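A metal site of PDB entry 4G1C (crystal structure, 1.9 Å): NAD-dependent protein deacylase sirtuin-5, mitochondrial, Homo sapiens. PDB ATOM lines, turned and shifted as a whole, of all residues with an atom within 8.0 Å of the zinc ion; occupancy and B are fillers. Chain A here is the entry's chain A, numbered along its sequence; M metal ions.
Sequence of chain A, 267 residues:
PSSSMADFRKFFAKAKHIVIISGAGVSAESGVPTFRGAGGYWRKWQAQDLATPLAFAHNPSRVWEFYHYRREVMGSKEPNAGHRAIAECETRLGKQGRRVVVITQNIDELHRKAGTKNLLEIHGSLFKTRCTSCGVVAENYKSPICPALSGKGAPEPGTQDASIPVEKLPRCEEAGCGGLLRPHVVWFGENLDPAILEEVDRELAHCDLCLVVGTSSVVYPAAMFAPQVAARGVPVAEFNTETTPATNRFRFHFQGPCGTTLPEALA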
ATOM      1  N   ARG A 130       9.553  16.397 -22.315  1.00  0.00           N
ATOM      2  CA  ARG A 130      10.392  17.580 -22.385  1.00  0.00           C
ATOM      3  C   ARG A 130      11.077  17.780 -21.050  1.00  0.00           C
ATOM      4  O   ARG A 130      10.463  17.639 -19.982  1.00  0.00           O
ATOM      5  CB  ARG A 130       9.576  18.821 -22.757  1.00  0.00           C
ATOM      6  CG  ARG A 130      10.452  20.067 -22.906  1.00  0.00           C
ATOM      7  CD  ARG A 130       9.739  21.219 -23.611  1.00  0.00           C
ATOM      8  NE  ARG A 130       8.894  22.046 -22.746  1.00  0.00           N
ATOM      9  CZ  ARG A 130       7.563  22.006 -22.732  1.00  0.00           C
ATOM     10  NH1 ARG A 130       6.906  21.143 -23.491  1.00  0.00           N
ATOM     11  NH2 ARG A 130       6.875  22.821 -21.946  1.00  0.00           N
ATOM     12  N   CYS A 131      12.361  18.104 -21.098  1.00  0.00           N
ATOM     13  CA  CYS A 131      13.096  18.329 -19.851  1.00  0.00           C
ATOM     14  C   CYS A 131      12.855  19.725 -19.287  1.00  0.00           C
ATOM     15  O   CYS A 131      13.109  20.726 -19.949  1.00  0.00           O
ATOM     16  CB  CYS A 131      14.596  18.107 -20.034  1.00  0.00           C
ATOM     17  SG  CYS A 131      15.458  18.505 -18.510  1.00  0.00           S
ATOM     18  N   THR A 132      12.400  19.770 -18.042  1.00  0.00           N
ATOM     19  CA  THR A 132      12.090  21.037 -17.392  1.00  0.00           C
ATOM     20  C   THR A 132      13.332  21.864 -17.018  1.00  0.00           C
ATOM     21  O   THR A 132      13.209  22.945 -16.474  1.00  0.00           O
ATOM     22  CB  THR A 132      11.233  20.821 -16.138  1.00  0.00           C
ATOM     23  OG1 THR A 132      11.994  20.134 -15.141  1.00  0.00           O
ATOM     24  CG2 THR A 132       9.998  19.988 -16.479  1.00  0.00           C
ATOM     25  N   SER A 133      14.529  21.335 -17.303  1.00  0.00           N
ATOM     26  CA  SER A 133      15.749  22.109 -17.060  1.00  0.00           C
ATOM     27  C   SER A 133      16.427  22.537 -18.355  1.00  0.00           C
ATOM     28  O   SER A 133      16.740  23.727 -18.552  1.00  0.00           O
ATOM     29  CB  SER A 133      16.744  21.327 -16.190  1.00  0.00           C
ATOM     30  OG  SER A 133      16.140  20.922 -14.976  1.00  0.00           O
ATOM     31  N   CYS A 134      16.649  21.593 -19.257  1.00  0.00           N
ATOM     32  CA  CYS A 134      17.368  21.909 -20.484  1.00  0.00           C
ATOM     33  C   CYS A 134      16.478  22.088 -21.712  1.00  0.00           C
ATOM     34  O   CYS A 134      16.941  22.563 -22.749  1.00  0.00           O
ATOM     35  CB  CYS A 134      18.513  20.912 -20.744  1.00  0.00           C
ATOM     36  SG  CYS A 134      18.027  19.204 -21.105  1.00  0.00           S
ATOM     37  N   GLY A 135      15.195  21.761 -21.586  1.00  0.00           N
ATOM     38  CA  GLY A 135      14.235  22.014 -22.656  1.00  0.00           C
ATOM     39  C   GLY A 135      14.268  21.016 -23.813  1.00  0.00           C
ATOM     40  O   GLY A 135      13.599  21.204 -24.841  1.00  0.00           O
ATOM     41  N   VAL A 136      15.046  19.951 -23.652  1.00  0.00           N
ATOM     42  CA  VAL A 136      15.174  18.990 -24.737  1.00  0.00           C
ATOM     43  C   VAL A 136      13.945  18.082 -24.854  1.00  0.00           C
ATOM     44  O   VAL A 136      13.467  17.509 -23.873  1.00  0.00           O
ATOM     45  CB  VAL A 136      16.485  18.170 -24.648  1.00  0.00           C
ATOM     46  CG1 VAL A 136      16.479  17.015 -25.660  1.00  0.00           C
ATOM     47  CG2 VAL A 136      17.669  19.088 -24.879  1.00  0.00           C
ATOM     48  N   VAL A 137      13.441  17.975 -26.074  1.00  0.00           N
ATOM     49  CA  VAL A 137      12.262  17.167 -26.343  1.00  0.00           C
ATOM     50  C   VAL A 137      12.686  15.848 -26.970  1.00  0.00           C
ATOM     51  O   VAL A 137      13.447  15.850 -27.923  1.00  0.00           O
ATOM     52  CB  VAL A 137      11.363  17.870 -27.347  1.00  0.00           C
ATOM     53  CG1 VAL A 137      10.221  16.951 -27.799  1.00  0.00           C
ATOM     54  CG2 VAL A 137      10.832  19.151 -26.744  1.00  0.00           C
ATOM     55  N   ARG A 171      13.521  11.063 -15.526  1.00  0.00           N
ATOM     56  CA  ARG A 171      14.628  12.022 -15.472  1.00  0.00           C
ATOM     57  C   ARG A 171      15.310  12.149 -16.818  1.00  0.00           C
ATOM     58  O   ARG A 171      15.374  11.180 -17.587  1.00  0.00           O
ATOM     59  CB  ARG A 171      15.665  11.590 -14.414  1.00  0.00           C
ATOM     60  CG  ARG A 171      15.105  11.339 -13.019  1.00  0.00           C
ATOM     61  CD  ARG A 171      14.334  12.529 -12.436  1.00  0.00           C
ATOM     62  NE  ARG A 171      15.142  13.753 -12.343  1.00  0.00           N
ATOM     63  CZ  ARG A 171      14.928  14.718 -11.451  1.00  0.00           C
ATOM     64  NH1 ARG A 171      13.943  14.601 -10.561  1.00  0.00           N
ATOM     65  NH2 ARG A 171      15.699  15.799 -11.450  1.00  0.00           N
ATOM     66  N   CYS A 172      15.816  13.343 -17.110  1.00  0.00           N
ATOM     67  CA  CYS A 172      16.498  13.617 -18.369  1.00  0.00           C
ATOM     68  C   CYS A 172      17.731  12.737 -18.456  1.00  0.00           C
ATOM     69  O   CYS A 172      18.437  12.554 -17.464  1.00  0.00           O
ATOM     70  CB  CYS A 172      16.929  15.066 -18.433  1.00  0.00           C
ATOM     71  SG  CYS A 172      17.486  15.614 -20.041  1.00  0.00           S
ATOM     72  N   GLU A 173      18.007  12.211 -19.643  1.00  0.00           N
ATOM     73  CA  GLU A 173      19.207  11.399 -19.831  1.00  0.00           C
ATOM     74  C   GLU A 173      20.169  12.095 -20.772  1.00  0.00           C
ATOM     75  O   GLU A 173      20.961  11.469 -21.464  1.00  0.00           O
ATOM     76  CB  GLU A 173      18.841  10.010 -20.359  1.00  0.00           C
ATOM     77  CG  GLU A 173      18.058   9.167 -19.353  1.00  0.00           C
ATOM     78  CD  GLU A 173      17.640   7.824 -19.922  1.00  0.00           C
ATOM     79  OE1 GLU A 173      17.816   7.608 -21.135  1.00  0.00           O
ATOM     80  OE2 GLU A 173      17.130   6.984 -19.146  1.00  0.00           O
ATOM     81  N   GLU A 174      20.083  13.429 -20.797  1.00  0.00           N
ATOM     82  CA  GLU A 174      21.012  14.233 -21.568  1.00  0.00           C
ATOM     83  C   GLU A 174      22.313  14.403 -20.783  1.00  0.00           C
ATOM     84  O   GLU A 174      22.316  14.315 -19.552  1.00  0.00           O
ATOM     85  CB  GLU A 174      20.410  15.598 -21.897  1.00  0.00           C
ATOM     86  CG  GLU A 174      20.938  16.228 -23.163  1.00  0.00           C
ATOM     87  CD  GLU A 174      20.393  15.580 -24.422  1.00  0.00           C
ATOM     88  OE1 GLU A 174      20.647  16.106 -25.518  1.00  0.00           O
ATOM     89  OE2 GLU A 174      19.695  14.545 -24.321  1.00  0.00           O
ATOM     90  N   ALA A 175      23.398  14.634 -21.504  1.00  0.00           N
ATOM     91  CA  ALA A 175      24.735  14.702 -20.911  1.00  0.00           C
ATOM     92  C   ALA A 175      24.837  15.745 -19.807  1.00  0.00           C
ATOM     93  O   ALA A 175      24.911  16.946 -20.071  1.00  0.00           O
ATOM     94  CB  ALA A 175      25.784  14.974 -21.999  1.00  0.00           C
ATOM     95  N   GLY A 176      24.836  15.268 -18.563  1.00  0.00           N
ATOM     96  CA  GLY A 176      25.057  16.142 -17.423  1.00  0.00           C
ATOM     97  C   GLY A 176      23.866  16.949 -16.951  1.00  0.00           C
ATOM     98  O   GLY A 176      24.022  17.888 -16.163  1.00  0.00           O
ATOM     99  N   CYS A 177      22.662  16.597 -17.424  1.00  0.00           N
ATOM    100  CA  CYS A 177      21.463  17.299 -16.976  1.00  0.00           C
ATOM    101  C   CYS A 177      20.806  16.660 -15.753  1.00  0.00           C
ATOM    102  O   CYS A 177      20.964  17.141 -14.632  1.00  0.00           O
ATOM    103  CB  CYS A 177      20.440  17.441 -18.113  1.00  0.00           C
ATOM    104  SG  CYS A 177      18.974  18.381 -17.595  1.00  0.00           S
ATOM    105  N   GLY A 178      20.075  15.568 -15.967  1.00  0.00           N
ATOM    106  CA  GLY A 178      19.389  14.882 -14.879  1.00  0.00           C
ATOM    107  C   GLY A 178      18.078  15.523 -14.457  1.00  0.00           C
ATOM    108  O   GLY A 178      17.480  15.118 -13.453  1.00  0.00           O
ATOM    109  N   GLY A 179      17.617  16.507 -15.222  1.00  0.00           N
ATOM    110  CA  GLY A 179      16.415  17.242 -14.881  1.00  0.00           C
ATOM    111  C   GLY A 179      15.155  16.412 -14.828  1.00  0.00           C
ATOM    112  O   GLY A 179      15.117  15.292 -15.344  1.00  0.00           O
ATOM    113  N   LEU A 180      14.125  16.937 -14.176  1.00  0.00           N
ATOM    114  CA  LEU A 180      12.830  16.287 -14.191  1.00  0.00           C
ATOM    115  C   LEU A 180      12.204  16.476 -15.561  1.00  0.00           C
ATOM    116  O   LEU A 180      12.192  17.581 -16.108  1.00  0.00           O
ATOM    117  CB  LEU A 180      11.908  16.868 -13.118  1.00  0.00           C
ATOM    118  CG  LEU A 180      10.448  16.387 -13.078  1.00  0.00           C
ATOM    119  CD1 LEU A 180      10.343  14.861 -12.945  1.00  0.00           C
ATOM    120  CD2 LEU A 180       9.674  17.082 -11.958  1.00  0.00           C
ATOM    121  N   LEU A 181      11.703  15.381 -16.129  1.00  0.00           N
ATOM    122  CA  LEU A 181      10.966  15.447 -17.376  1.00  0.00           C
ATOM    123  C   LEU A 181       9.526  15.727 -17.068  1.00  0.00           C
ATOM    124  O   LEU A 181       9.041  15.501 -15.951  1.00  0.00           O
ATOM    125  CB  LEU A 181      11.050  14.125 -18.148  1.00  0.00           C
ATOM    126  CG  LEU A 181      12.458  13.699 -18.561  1.00  0.00           C
ATOM    127  CD1 LEU A 181      12.420  12.398 -19.366  1.00  0.00           C
ATOM    128  CD2 LEU A 181      13.097  14.820 -19.363  1.00  0.00           C
HETATM  129 ZN    ZN M   1      17.613  17.945 -19.493  1.00  0.00          ZN
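The zinc ion is bound by the side-chain sulfur of Cys 134, the side-chain sulfur of Cys 177, the side-chain sulfur of Cys 172 and the side-chain sulfur of Cys 131.
Of the 19 residues printed, 4 come within 4 Å of the zinc ion. The nearest printed residue that does not touch the zinc ion is Glu 174 (4.4 Å).
O of Gly 179 is in hydrogen-bond range of N of Cys 172 (2.7 Å). N of Ser 133 lies close to SG of Cys 131 (3.2 Å). N of Gly 179 lies close to SG of Cys 177. The backbone NH of Cys 131 is in hydrogen-bond range of the backbone carbonyl oxygen of Val 136, at 3.0 Å. The backbone NH of Glu 174 sits close to the side-chain sulfur of Cys 172, 3.5 Å away.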
